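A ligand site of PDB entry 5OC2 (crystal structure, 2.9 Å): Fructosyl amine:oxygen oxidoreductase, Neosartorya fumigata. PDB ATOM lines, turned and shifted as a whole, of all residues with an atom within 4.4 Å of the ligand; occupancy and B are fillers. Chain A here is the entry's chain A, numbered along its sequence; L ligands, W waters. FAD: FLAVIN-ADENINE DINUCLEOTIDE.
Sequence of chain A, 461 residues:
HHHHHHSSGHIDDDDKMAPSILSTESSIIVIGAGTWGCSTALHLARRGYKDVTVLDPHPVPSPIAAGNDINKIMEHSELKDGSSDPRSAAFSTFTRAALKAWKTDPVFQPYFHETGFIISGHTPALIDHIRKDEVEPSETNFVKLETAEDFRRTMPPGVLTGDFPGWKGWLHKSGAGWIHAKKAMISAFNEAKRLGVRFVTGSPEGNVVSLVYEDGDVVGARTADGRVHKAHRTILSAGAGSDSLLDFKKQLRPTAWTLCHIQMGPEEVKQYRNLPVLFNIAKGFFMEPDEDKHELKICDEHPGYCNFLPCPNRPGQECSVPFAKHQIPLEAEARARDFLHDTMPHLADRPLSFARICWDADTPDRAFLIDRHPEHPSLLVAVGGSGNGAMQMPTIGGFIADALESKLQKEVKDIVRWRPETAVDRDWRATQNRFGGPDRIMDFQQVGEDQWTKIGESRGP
The backbone NH (N) of Ala 66 sits at hydrogen-bond distance from an oxygen (O1A) of the ligand (2.5 Å). The backbone carbonyl oxygen (O) of Ala 66 lies close to an oxygen (O2') of the ligand, 3.1 Å away. An oxygen (O4) of the ligand sits at hydrogen-bond distance from the backbone NH (N) of Ile 73, at 2.6 Å. O of Ile 73 is in hydrogen-bond range of N3 of the ligand (2.8 Å). O3B of the ligand lies within hydrogen-bond range of OD2 of Asp 56. The backbone NH (N) of Thr 35 sits close to an oxygen (O1P) of the ligand (3.1 Å). The side-chain hydroxyl of Thr 35 lies within hydrogen-bond range of an oxygen (O2A) of the ligand, at 2.6 Å. An oxygen (O1P) of the ligand is in hydrogen-bond range of the backbone NH of Trp 36 (2.8 Å). N of Val 208 is in hydrogen-bond range of N1A of the ligand (3.2 Å). N6A of the ligand sits at hydrogen-bond distance from O of Val 208 (2.8 Å). An oxygen (O2B) of the ligand is in hydrogen-bond range of the side-chain hydroxyl (OG) of Ser 62 (2.8 Å). O2 of the ligand sits at hydrogen-bond distance from N of Met 391 (2.8 Å). An oxygen (O4') of the ligand sits at hydrogen-bond distance from the side-chain carboxylate of Asp 360, at 3.0 Å. N of Ala 390 lies within hydrogen-bond range of O2 of the ligand, 3.0 Å away. The backbone NH (N) of Gly 67 is in hydrogen-bond range of an oxygen (O2A) of the ligand (3.2 Å). The backbone NH (N) of Gly 389 is in hydrogen-bond range of a nitrogen (N1) of the ligand.
The backbone carbonyl oxygen of Gly 206 sits close to the backbone NH of Asp 56, 3.3 Å away. The side-chain hydroxyl (OG1) of Thr 35 lies close to the backbone NH (N) of Gly 67. NE1 of Trp 36 is in hydrogen-bond range of O of Gly 389 (2.9 Å). OG of Ser 62 sits close to N of Ile 64, 3.5 Å away. The backbone NH (N) of Gly 387 is in hydrogen-bond range of the side-chain carboxylate (OD2) of Asp 360 (2.7 Å). The backbone carbonyl oxygen (O) of Cys 358 sits at hydrogen-bond distance from the backbone NH (N) of Trp 257, at 2.7 Å. The backbone carbonyl oxygen (O) of Ile 31 sits at hydrogen-bond distance from the backbone NH (N) of Ser 237, at 2.9 Å. The backbone carbonyl oxygen (O) of Gly 32 sits at hydrogen-bond distance from the side-chain hydroxyl (OG) of Ser 237 (3.4 Å).
The backbone carbonyl oxygen (O) of Ala 238 sits close to an oxygen (O4B) of the ligand, 3.4 Å away. O of Gly 387 lies close to N1 of the ligand (3.0 Å). O2 of the ligand sits close to O of Asn 388. Residues that only touch the ligand: Ile 31, Gly 32, Ala 33, Gly 34, Leu 55, Pro 57, His 58, Ile 64, Ala 65, Lys 72, Asn 207, Ser 237, Gly 239, Leu 245, Trp 257, Cys 358 and Gly 385.
Water W3 lies within hydrogen-bond range of the backbone NH (N) of Gly 239 (2.5 Å), an oxygen (O2P) of the ligand (2.7 Å) and the backbone NH (N) of Ala 238 (3.0 Å). Water W2 lies within hydrogen-bond range of O1A of the ligand (2.8 Å) and O of Trp 359 (2.8 Å). Water W1 lies within hydrogen-bond range of the backbone carbonyl oxygen of Ser 237 (2.9 Å), an oxygen (O1P) of the ligand (2.9 Å), the backbone NH of Gly 34 (3.1 Å) and the backbone NH of Trp 36 (3.4 Å). Water W4 lies within hydrogen-bond range of the side-chain carboxylate of Asp 360, the backbone NH of Gly 385 and an oxygen (O5') of the ligand.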
ATOM      1  N   ILE A  31      15.586 -32.022  26.248  1.00  0.00           N
ATOM      2  CA  ILE A  31      15.826 -31.069  27.318  1.00  0.00           C
ATOM      3  C   ILE A  31      16.641 -29.908  26.772  1.00  0.00           C
ATOM      4  O   ILE A  31      17.816 -30.065  26.466  1.00  0.00           O
ATOM      5  CB  ILE A  31      16.619 -31.697  28.463  1.00  0.00           C
ATOM      6  CG1 ILE A  31      16.013 -33.038  28.897  1.00  0.00           C
ATOM      7  CG2 ILE A  31      16.731 -30.716  29.634  1.00  0.00           C
ATOM      8  CD1 ILE A  31      16.757 -33.661  30.051  1.00  0.00           C
ATOM      9  N   GLY A  32      16.015 -28.750  26.633  1.00  0.00           N
ATOM     10  CA  GLY A  32      16.678 -27.599  26.041  1.00  0.00           C
ATOM     11  C   GLY A  32      16.123 -27.220  24.673  1.00  0.00           C
ATOM     12  O   GLY A  32      16.245 -27.974  23.717  1.00  0.00           O
ATOM     13  N   ALA A  33      15.516 -26.031  24.578  1.00  0.00           N
ATOM     14  CA  ALA A  33      15.047 -25.531  23.289  1.00  0.00           C
ATOM     15  C   ALA A  33      15.886 -24.331  22.796  1.00  0.00           C
ATOM     16  O   ALA A  33      15.343 -23.288  22.426  1.00  0.00           O
ATOM     17  CB  ALA A  33      13.568 -25.163  23.358  1.00  0.00           C
ATOM     18  N   GLY A  34      17.204 -24.510  22.811  1.00  0.00           N
ATOM     19  CA  GLY A  34      18.120 -23.537  22.243  1.00  0.00           C
ATOM     20  C   GLY A  34      18.456 -23.856  20.801  1.00  0.00           C
ATOM     21  O   GLY A  34      17.621 -24.407  20.068  1.00  0.00           O
ATOM     22  N   THR A  35      19.675 -23.506  20.383  1.00  0.00           N
ATOM     23  CA  THR A  35      20.159 -23.756  19.030  1.00  0.00           C
ATOM     24  C   THR A  35      19.891 -25.194  18.620  1.00  0.00           C
ATOM     25  O   THR A  35      19.113 -25.477  17.708  1.00  0.00           O
ATOM     26  CB  THR A  35      21.692 -23.503  18.930  1.00  0.00           C
ATOM     27  OG1 THR A  35      22.060 -22.391  19.758  1.00  0.00           O
ATOM     28  CG2 THR A  35      22.111 -23.246  17.495  1.00  0.00           C
ATOM     29  N   TRP A  36      20.515 -26.107  19.351  1.00  0.00           N
ATOM     30  CA  TRP A  36      20.499 -27.533  19.041  1.00  0.00           C
ATOM     31  C   TRP A  36      19.188 -28.234  19.370  1.00  0.00           C
ATOM     32  O   TRP A  36      18.803 -29.214  18.714  1.00  0.00           O
ATOM     33  CB  TRP A  36      21.661 -28.205  19.769  1.00  0.00           C
ATOM     34  CG  TRP A  36      22.999 -27.849  19.166  1.00  0.00           C
ATOM     35  CD1 TRP A  36      23.258 -26.811  18.316  1.00  0.00           C
ATOM     36  CD2 TRP A  36      24.240 -28.542  19.349  1.00  0.00           C
ATOM     37  NE1 TRP A  36      24.581 -26.818  17.959  1.00  0.00           N
ATOM     38  CE2 TRP A  36      25.204 -27.866  18.583  1.00  0.00           C
ATOM     39  CE3 TRP A  36      24.619 -29.674  20.084  1.00  0.00           C
ATOM     40  CZ2 TRP A  36      26.546 -28.277  18.530  1.00  0.00           C
ATOM     41  CZ3 TRP A  36      25.941 -30.078  20.026  1.00  0.00           C
ATOM     42  CH2 TRP A  36      26.888 -29.385  19.256  1.00  0.00           C
ATOM     43  N   LEU A  55      11.485 -29.491  26.440  1.00  0.00           N
ATOM     44  CA  LEU A  55      11.455 -28.808  27.737  1.00  0.00           C
ATOM     45  C   LEU A  55      12.481 -27.680  27.849  1.00  0.00           C
ATOM     46  O   LEU A  55      13.650 -27.875  27.526  1.00  0.00           O
ATOM     47  CB  LEU A  55      11.654 -29.827  28.878  1.00  0.00           C
ATOM     48  CG  LEU A  55      10.619 -30.973  28.930  1.00  0.00           C
ATOM     49  CD1 LEU A  55      10.996 -32.056  29.954  1.00  0.00           C
ATOM     50  CD2 LEU A  55       9.215 -30.456  29.220  1.00  0.00           C
ATOM     51  N   ASP A  56      12.051 -26.485  28.270  1.00  0.00           N
ATOM     52  CA  ASP A  56      12.979 -25.365  28.522  1.00  0.00           C
ATOM     53  C   ASP A  56      12.429 -24.427  29.610  1.00  0.00           C
ATOM     54  O   ASP A  56      11.222 -24.175  29.661  1.00  0.00           O
ATOM     55  CB  ASP A  56      13.248 -24.572  27.244  1.00  0.00           C
ATOM     56  CG  ASP A  56      14.545 -23.758  27.310  1.00  0.00           C
ATOM     57  OD1 ASP A  56      14.636 -22.821  28.126  1.00  0.00           O
ATOM     58  OD2 ASP A  56      15.475 -24.073  26.524  1.00  0.00           O
ATOM     59  N   PRO A  57      13.313 -23.929  30.480  1.00  0.00           N
ATOM     60  CA  PRO A  57      12.828 -23.065  31.574  1.00  0.00           C
ATOM     61  C   PRO A  57      12.428 -21.680  31.074  1.00  0.00           C
ATOM     62  O   PRO A  57      11.804 -20.922  31.843  1.00  0.00           O
ATOM     63  CB  PRO A  57      14.031 -22.994  32.513  1.00  0.00           C
ATOM     64  CG  PRO A  57      15.214 -23.340  31.664  1.00  0.00           C
ATOM     65  CD  PRO A  57      14.729 -24.307  30.657  1.00  0.00           C
ATOM     66  N   HIS A  58      12.771 -21.360  29.830  1.00  0.00           N
ATOM     67  CA  HIS A  58      12.467 -20.055  29.205  1.00  0.00           C
ATOM     68  C   HIS A  58      11.738 -20.183  27.859  1.00  0.00           C
ATOM     69  O   HIS A  58      11.935 -21.159  27.128  1.00  0.00           O
ATOM     70  CB  HIS A  58      13.752 -19.244  28.994  1.00  0.00           C
ATOM     71  CG  HIS A  58      14.559 -19.053  30.234  1.00  0.00           C
ATOM     72  ND1 HIS A  58      14.196 -18.174  31.236  1.00  0.00           N
ATOM     73  CD2 HIS A  58      15.703 -19.650  30.659  1.00  0.00           C
ATOM     74  CE1 HIS A  58      15.083 -18.229  32.210  1.00  0.00           C
ATOM     75  NE2 HIS A  58      16.009 -19.119  31.888  1.00  0.00           N
ATOM     76  N   SER A  62      15.520 -18.163  24.446  1.00  0.00           N
ATOM     77  CA  SER A  62      15.933 -18.142  25.852  1.00  0.00           C
ATOM     78  C   SER A  62      16.985 -17.058  26.085  1.00  0.00           C
ATOM     79  O   SER A  62      17.903 -16.880  25.278  1.00  0.00           O
ATOM     80  CB  SER A  62      16.446 -19.522  26.280  1.00  0.00           C
ATOM     81  OG  SER A  62      16.755 -19.549  27.665  1.00  0.00           O
ATOM     82  N   ILE A  64      19.257 -17.181  28.125  1.00  0.00           N
ATOM     83  CA  ILE A  64      20.527 -17.829  28.466  1.00  0.00           C
ATOM     84  C   ILE A  64      21.035 -18.739  27.349  1.00  0.00           C
ATOM     85  O   ILE A  64      22.142 -19.261  27.433  1.00  0.00           O
ATOM     86  CB  ILE A  64      20.456 -18.637  29.788  1.00  0.00           C
ATOM     87  CG1 ILE A  64      19.681 -19.941  29.598  1.00  0.00           C
ATOM     88  CG2 ILE A  64      19.876 -17.775  30.888  1.00  0.00           C
ATOM     89  CD1 ILE A  64      19.514 -20.743  30.866  1.00  0.00           C
ATOM     90  N   ALA A  65      20.216 -18.921  26.319  1.00  0.00           N
ATOM     91  CA  ALA A  65      20.648 -19.685  25.150  1.00  0.00           C
ATOM     92  C   ALA A  65      21.719 -18.907  24.393  1.00  0.00           C
ATOM     93  O   ALA A  65      21.532 -17.727  24.055  1.00  0.00           O
ATOM     94  CB  ALA A  65      19.464 -19.995  24.225  1.00  0.00           C
ATOM     95  N   ALA A  66      22.839 -19.561  24.151  1.00  0.00           N
ATOM     96  CA  ALA A  66      23.904 -18.956  23.354  1.00  0.00           C
ATOM     97  C   ALA A  66      23.495 -18.697  21.896  1.00  0.00           C
ATOM     98  O   ALA A  66      24.135 -17.917  21.208  1.00  0.00           O
ATOM     99  CB  ALA A  66      25.146 -19.835  23.410  1.00  0.00           C
ATOM    100  N   GLY A  67      22.430 -19.346  21.435  1.00  0.00           N
ATOM    101  CA  GLY A  67      21.968 -19.167  20.075  1.00  0.00           C
ATOM    102  C   GLY A  67      21.185 -17.873  19.918  1.00  0.00           C
ATOM    103  O   GLY A  67      20.934 -17.389  18.803  1.00  0.00           O
ATOM    104  N   LYS A  72      25.552 -14.512  14.175  1.00  0.00           N
ATOM    105  CA  LYS A  72      26.672 -15.436  14.400  1.00  0.00           C
ATOM    106  C   LYS A  72      27.349 -15.698  13.071  1.00  0.00           C
ATOM    107  O   LYS A  72      26.731 -15.552  12.034  1.00  0.00           O
ATOM    108  CB  LYS A  72      26.178 -16.768  14.981  1.00  0.00           C
ATOM    109  CG  LYS A  72      25.418 -16.699  16.289  1.00  0.00           C
ATOM    110  CD  LYS A  72      26.329 -16.427  17.463  1.00  0.00           C
ATOM    111  CE  LYS A  72      25.741 -16.991  18.739  1.00  0.00           C
ATOM    112  NZ  LYS A  72      26.254 -16.254  19.916  1.00  0.00           N
ATOM    113  N   ILE A  73      28.609 -16.106  13.117  1.00  0.00           N
ATOM    114  CA  ILE A  73      29.365 -16.418  11.909  1.00  0.00           C
ATOM    115  C   ILE A  73      29.054 -17.821  11.410  1.00  0.00           C
ATOM    116  O   ILE A  73      29.020 -18.764  12.194  1.00  0.00           O
ATOM    117  CB  ILE A  73      30.890 -16.346  12.180  1.00  0.00           C
ATOM    118  CG1 ILE A  73      31.283 -15.004  12.787  1.00  0.00           C
ATOM    119  CG2 ILE A  73      31.688 -16.643  10.905  1.00  0.00           C
ATOM    120  CD1 ILE A  73      32.665 -15.002  13.392  1.00  0.00           C
ATOM    121  N   GLY A 206       8.781 -26.230  32.552  1.00  0.00           N
ATOM    122  CA  GLY A 206       9.814 -26.722  31.653  1.00  0.00           C
ATOM    123  C   GLY A 206      11.237 -26.673  32.197  1.00  0.00           C
ATOM    124  O   GLY A 206      12.193 -27.119  31.547  1.00  0.00           O
ATOM    125  N   ASN A 207      11.397 -26.144  33.400  1.00  0.00           N
ATOM    126  CA  ASN A 207      12.716 -26.101  34.003  1.00  0.00           C
ATOM    127  C   ASN A 207      13.069 -27.478  34.565  1.00  0.00           C
ATOM    128  O   ASN A 207      12.564 -27.870  35.619  1.00  0.00           O
ATOM    129  CB  ASN A 207      12.777 -25.039  35.085  1.00  0.00           C
ATOM    130  CG  ASN A 207      14.126 -24.969  35.739  1.00  0.00           C
ATOM    131  OD1 ASN A 207      15.157 -25.210  35.113  1.00  0.00           O
ATOM    132  ND2 ASN A 207      14.131 -24.646  37.037  1.00  0.00           N
ATOM    133  N   VAL A 208      13.931 -28.204  33.861  1.00  0.00           N
ATOM    134  CA  VAL A 208      14.313 -29.557  34.246  1.00  0.00           C
ATOM    135  C   VAL A 208      15.366 -29.513  35.352  1.00  0.00           C
ATOM    136  O   VAL A 208      16.446 -28.958  35.173  1.00  0.00           O
ATOM    137  CB  VAL A 208      14.855 -30.352  33.040  1.00  0.00           C
ATOM    138  CG1 VAL A 208      14.905 -31.833  33.349  1.00  0.00           C
ATOM    139  CG2 VAL A 208      14.002 -30.098  31.828  1.00  0.00           C
ATOM    140  N   SER A 237      20.097 -31.520  25.523  1.00  0.00           N
ATOM    141  CA  SER A 237      20.765 -30.465  24.757  1.00  0.00           C
ATOM    142  C   SER A 237      20.574 -29.105  25.444  1.00  0.00           C
ATOM    143  O   SER A 237      19.859 -28.241  24.927  1.00  0.00           O
ATOM    144  CB  SER A 237      20.183 -30.380  23.361  1.00  0.00           C
ATOM    145  OG  SER A 237      18.769 -30.278  23.443  1.00  0.00           O
ATOM    146  N   ALA A 238      21.203 -28.911  26.604  1.00  0.00           N
ATOM    147  CA  ALA A 238      20.954 -27.700  27.367  1.00  0.00           C
ATOM    148  C   ALA A 238      22.107 -26.673  27.374  1.00  0.00           C
ATOM    149  O   ALA A 238      22.148 -25.801  28.239  1.00  0.00           O
ATOM    150  CB  ALA A 238      20.549 -28.043  28.783  1.00  0.00           C
ATOM    151  N   GLY A 239      23.013 -26.766  26.396  1.00  0.00           N
ATOM    152  CA  GLY A 239      24.125 -25.842  26.309  1.00  0.00           C
ATOM    153  C   GLY A 239      24.923 -25.865  27.595  1.00  0.00           C
ATOM    154  O   GLY A 239      25.157 -26.950  28.149  1.00  0.00           O
ATOM    155  N   GLY A 241      24.150 -25.236  30.465  1.00  0.00           N
ATOM    156  CA  GLY A 241      23.382 -25.744  31.587  1.00  0.00           C
ATOM    157  C   GLY A 241      23.415 -27.251  31.719  1.00  0.00           C
ATOM    158  O   GLY A 241      23.005 -27.777  32.751  1.00  0.00           O
ATOM    159  N   LEU A 245      23.260 -31.422  35.136  1.00  0.00           N
ATOM    160  CA  LEU A 245      22.147 -32.354  34.953  1.00  0.00           C
ATOM    161  C   LEU A 245      22.631 -33.794  34.746  1.00  0.00           C
ATOM    162  O   LEU A 245      21.849 -34.741  34.767  1.00  0.00           O
ATOM    163  CB  LEU A 245      21.299 -31.915  33.763  1.00  0.00           C
ATOM    164  CG  LEU A 245      20.196 -30.888  34.029  1.00  0.00           C
ATOM    165  CD1 LEU A 245      19.557 -30.436  32.711  1.00  0.00           C
ATOM    166  CD2 LEU A 245      19.135 -31.449  34.968  1.00  0.00           C
ATOM    167  N   TRP A 257      31.770 -15.905  26.840  1.00  0.00           N
ATOM    168  CA  TRP A 257      32.376 -14.857  26.043  1.00  0.00           C
ATOM    169  C   TRP A 257      31.520 -13.576  26.093  1.00  0.00           C
ATOM    170  O   TRP A 257      30.355 -13.614  26.496  1.00  0.00           O
ATOM    171  CB  TRP A 257      32.648 -15.325  24.605  1.00  0.00           C
ATOM    172  CG  TRP A 257      33.862 -16.231  24.527  1.00  0.00           C
ATOM    173  CD1 TRP A 257      35.141 -15.853  24.238  1.00  0.00           C
ATOM    174  CD2 TRP A 257      33.890 -17.642  24.749  1.00  0.00           C
ATOM    175  NE1 TRP A 257      35.972 -16.944  24.258  1.00  0.00           N
ATOM    176  CE2 TRP A 257      35.233 -18.058  24.572  1.00  0.00           C
ATOM    177  CE3 TRP A 257      32.927 -18.593  25.093  1.00  0.00           C
ATOM    178  CZ2 TRP A 257      35.621 -19.385  24.723  1.00  0.00           C
ATOM    179  CZ3 TRP A 257      33.311 -19.896  25.239  1.00  0.00           C
ATOM    180  CH2 TRP A 257      34.648 -20.289  25.056  1.00  0.00           C
ATOM    181  N   CYS A 299      32.383  -8.632  19.577  1.00  0.00           N
ATOM    182  CA  CYS A 299      32.914  -9.547  20.552  1.00  0.00           C
ATOM    183  C   CYS A 299      34.409  -9.265  20.660  1.00  0.00           C
ATOM    184  O   CYS A 299      35.096  -9.200  19.648  1.00  0.00           O
ATOM    185  CB  CYS A 299      32.727 -11.006  20.103  1.00  0.00           C
ATOM    186  SG  CYS A 299      31.021 -11.655  20.090  1.00  0.00           S
ATOM    187  N   CYS A 358      27.912 -14.479  27.560  1.00  0.00           N
ATOM    188  CA  CYS A 358      27.330 -15.511  26.724  1.00  0.00           C
ATOM    189  C   CYS A 358      28.023 -16.832  26.985  1.00  0.00           C
ATOM    190  O   CYS A 358      29.252 -16.925  26.877  1.00  0.00           O
ATOM    191  CB  CYS A 358      27.480 -15.110  25.241  1.00  0.00           C
ATOM    192  SG  CYS A 358      26.578 -16.137  24.082  1.00  0.00           S
ATOM    193  N   TRP A 359      27.233 -17.849  27.326  1.00  0.00           N
ATOM    194  CA  TRP A 359      27.743 -19.139  27.813  1.00  0.00           C
ATOM    195  C   TRP A 359      27.704 -20.289  26.793  1.00  0.00           C
ATOM    196  O   TRP A 359      26.649 -20.602  26.237  1.00  0.00           O
ATOM    197  CB  TRP A 359      27.014 -19.531  29.093  1.00  0.00           C
ATOM    198  CG  TRP A 359      27.429 -18.733  30.279  1.00  0.00           C
ATOM    199  CD1 TRP A 359      26.839 -17.590  30.762  1.00  0.00           C
ATOM    200  CD2 TRP A 359      28.562 -18.990  31.140  1.00  0.00           C
ATOM    201  NE1 TRP A 359      27.521 -17.132  31.867  1.00  0.00           N
ATOM    202  CE2 TRP A 359      28.578 -17.965  32.120  1.00  0.00           C
ATOM    203  CE3 TRP A 359      29.548 -19.995  31.168  1.00  0.00           C
ATOM    204  CZ2 TRP A 359      29.554 -17.914  33.118  1.00  0.00           C
ATOM    205  CZ3 TRP A 359      30.513 -19.940  32.158  1.00  0.00           C
ATOM    206  CH2 TRP A 359      30.506 -18.906  33.123  1.00  0.00           C
ATOM    207  N   ASP A 360      28.856 -20.926  26.579  1.00  0.00           N
ATOM    208  CA  ASP A 360      28.936 -22.179  25.829  1.00  0.00           C
ATOM    209  C   ASP A 360      29.592 -23.267  26.688  1.00  0.00           C
ATOM    210  O   ASP A 360      29.842 -23.070  27.866  1.00  0.00           O
ATOM    211  CB  ASP A 360      29.700 -22.005  24.513  1.00  0.00           C
ATOM    212  CG  ASP A 360      29.187 -22.952  23.411  1.00  0.00           C
ATOM    213  OD1 ASP A 360      28.395 -23.898  23.703  1.00  0.00           O
ATOM    214  OD2 ASP A 360      29.577 -22.751  22.240  1.00  0.00           O
ATOM    215  N   GLY A 385      29.002 -27.427  21.965  1.00  0.00           N
ATOM    216  CA  GLY A 385      29.105 -26.663  20.743  1.00  0.00           C
ATOM    217  C   GLY A 385      30.470 -26.033  20.597  1.00  0.00           C
ATOM    218  O   GLY A 385      30.924 -25.764  19.479  1.00  0.00           O
ATOM    219  N   GLY A 387      31.865 -23.142  20.881  1.00  0.00           N
ATOM    220  CA  GLY A 387      32.077 -21.912  20.138  1.00  0.00           C
ATOM    221  C   GLY A 387      31.701 -21.967  18.657  1.00  0.00           C
ATOM    222  O   GLY A 387      31.699 -20.941  17.978  1.00  0.00           O
ATOM    223  N   ASN A 388      31.380 -23.157  18.168  1.00  0.00           N
ATOM    224  CA  ASN A 388      31.115 -23.392  16.748  1.00  0.00           C
ATOM    225  C   ASN A 388      29.758 -24.025  16.478  1.00  0.00           C
ATOM    226  O   ASN A 388      29.556 -24.644  15.431  1.00  0.00           O
ATOM    227  CB  ASN A 388      32.208 -24.302  16.164  1.00  0.00           C
ATOM    228  CG  ASN A 388      33.538 -23.608  16.016  1.00  0.00           C
ATOM    229  OD1 ASN A 388      33.630 -22.555  15.386  1.00  0.00           O
ATOM    230  ND2 ASN A 388      34.571 -24.182  16.621  1.00  0.00           N
ATOM    231  N   GLY A 389      28.836 -23.891  17.425  1.00  0.00           N
ATOM    232  CA  GLY A 389      27.578 -24.614  17.369  1.00  0.00           C
ATOM    233  C   GLY A 389      26.417 -23.900  16.731  1.00  0.00           C
ATOM    234  O   GLY A 389      25.436 -24.539  16.391  1.00  0.00           O
ATOM    235  N   ALA A 390      26.494 -22.584  16.575  1.00  0.00           N
ATOM    236  CA  ALA A 390      25.353 -21.804  16.121  1.00  0.00           C
ATOM    237  C   ALA A 390      25.101 -21.972  14.629  1.00  0.00           C
ATOM    238  O   ALA A 390      23.953 -22.068  14.181  1.00  0.00           O
ATOM    239  CB  ALA A 390      25.556 -20.348  16.464  1.00  0.00           C
ATOM    240  N   MET A 391      26.191 -22.014  13.874  1.00  0.00           N
ATOM    241  CA  MET A 391      26.132 -22.098  12.413  1.00  0.00           C
ATOM    242  C   MET A 391      25.559 -23.439  11.993  1.00  0.00           C
ATOM    243  O   MET A 391      25.154 -23.611  10.848  1.00  0.00           O
ATOM    244  CB  MET A 391      27.522 -21.927  11.807  1.00  0.00           C
ATOM    245  CG  MET A 391      28.481 -23.058  12.147  1.00  0.00           C
ATOM    246  SD  MET A 391      30.158 -22.887  11.489  1.00  0.00           S
ATOM    247  CE  MET A 391      30.784 -21.429  12.354  1.00  0.00           C
HETATM  248  PA  FAD L   1      22.042 -22.989  23.670  1.00  0.00           P
HETATM  249  O1A FAD L   1      22.587 -21.998  24.671  1.00  0.00           O
HETATM  250  O2A FAD L   1      21.767 -22.315  22.356  1.00  0.00           O
HETATM  251  O5B FAD L   1      20.659 -23.610  24.223  1.00  0.00           O
HETATM  252  C5B FAD L   1      20.605 -23.997  25.598  1.00  0.00           C
HETATM  253  C4B FAD L   1      19.164 -24.112  25.965  1.00  0.00           C
HETATM  254  O4B FAD L   1      19.027 -25.132  27.043  1.00  0.00           O
HETATM  255  C3B FAD L   1      18.692 -22.829  26.462  1.00  0.00           C
HETATM  256  O3B FAD L   1      17.432 -22.508  25.842  1.00  0.00           O
HETATM  257  C2B FAD L   1      18.537 -23.015  27.933  1.00  0.00           C
HETATM  258  O2B FAD L   1      17.545 -22.115  28.507  1.00  0.00           O
HETATM  259  C1B FAD L   1      18.196 -24.432  28.046  1.00  0.00           C
HETATM  260  N9A FAD L   1      18.368 -24.915  29.363  1.00  0.00           N
HETATM  261  C8A FAD L   1      19.144 -24.587  30.261  1.00  0.00           C
HETATM  262  N7A FAD L   1      19.089 -25.061  31.239  1.00  0.00           N
HETATM  263  C5A FAD L   1      18.291 -25.885  31.492  1.00  0.00           C
HETATM  264  C6A FAD L   1      17.625 -26.908  32.502  1.00  0.00           C
HETATM  265  N6A FAD L   1      18.086 -27.087  33.861  1.00  0.00           N
HETATM  266  N1A FAD L   1      16.524 -27.660  32.018  1.00  0.00           N
HETATM  267  C2A FAD L   1      16.157 -27.479  30.827  1.00  0.00           C
HETATM  268  N3A FAD L   1      16.575 -26.771  30.013  1.00  0.00           N
HETATM  269  C4A FAD L   1      17.482 -25.998  30.060  1.00  0.00           C
HETATM  270  N1  FAD L   1      28.860 -20.549  17.093  1.00  0.00           N
HETATM  271  C2  FAD L   1      28.957 -20.462  15.634  1.00  0.00           C
HETATM  272  O2  FAD L   1      28.756 -21.469  14.981  1.00  0.00           O
HETATM  273  N3  FAD L   1      29.283 -19.205  14.978  1.00  0.00           N
HETATM  274  C4  FAD L   1      29.521 -18.057  15.754  1.00  0.00           C
HETATM  275  O4  FAD L   1      29.804 -16.982  15.227  1.00  0.00           O
HETATM  276  C4X FAD L   1      29.423 -18.155  17.221  1.00  0.00           C
HETATM  277  N5  FAD L   1      29.639 -17.078  17.946  1.00  0.00           N
HETATM  278  C5X FAD L   1      29.528 -17.170  19.396  1.00  0.00           C
HETATM  279  C6  FAD L   1      29.757 -16.032  20.192  1.00  0.00           C
HETATM  280  C7  FAD L   1      29.646 -16.118  21.591  1.00  0.00           C
HETATM  281  C7M FAD L   1      29.901 -14.874  22.413  1.00  0.00           C
HETATM  282  C8  FAD L   1      29.323 -17.346  22.180  1.00  0.00           C
HETATM  283  C8M FAD L   1      29.245 -17.557  23.736  1.00  0.00           C
HETATM  284  C9  FAD L   1      29.127 -18.466  21.412  1.00  0.00           C
HETATM  285  C9A FAD L   1      29.211 -18.392  20.005  1.00  0.00           C
HETATM  286  N10 FAD L   1      28.990 -19.557  19.233  1.00  0.00           N
HETATM  287  C10 FAD L   1      29.080 -19.457  17.861  1.00  0.00           C
HETATM  288  C1' FAD L   1      28.614 -20.815  19.857  1.00  0.00           C
HETATM  289  C2' FAD L   1      27.071 -20.650  19.767  1.00  0.00           C
HETATM  290  O2' FAD L   1      26.586 -19.841  20.789  1.00  0.00           O
HETATM  291  C3' FAD L   1      26.192 -21.888  19.733  1.00  0.00           C
HETATM  292  O3' FAD L   1      24.850 -21.476  19.693  1.00  0.00           O
HETATM  293  C4' FAD L   1      26.269 -22.791  20.938  1.00  0.00           C
HETATM  294  O4' FAD L   1      27.283 -23.709  20.615  1.00  0.00           O
HETATM  295  C5' FAD L   1      24.840 -23.353  21.045  1.00  0.00           C
HETATM  296  O5' FAD L   1      24.678 -24.708  21.478  1.00  0.00           O
HETATM  297  P   FAD L   1      23.331 -25.151  22.284  1.00  0.00           P
HETATM  298  O1P FAD L   1      22.062 -25.159  21.441  1.00  0.00           O
HETATM  299  O2P FAD L   1      23.562 -26.547  22.802  1.00  0.00           O
HETATM  300  O3P FAD L   1      23.129 -24.175  23.533  1.00  0.00           O
HETATM  301  O   HOH W   1      19.715 -26.395  22.688  1.00  0.00           O
HETATM  302  O   HOH W   2      24.697 -22.617  26.361  1.00  0.00           O
HETATM  303  O   HOH W   3      23.491 -28.476  24.642  1.00  0.00           O
HETATM  304  O   HOH W   4      26.595 -26.256  23.312  1.00  0.00           O
HETATM  305  O   HOH W   5      20.500 -25.700  34.200  1.00  0.00           O
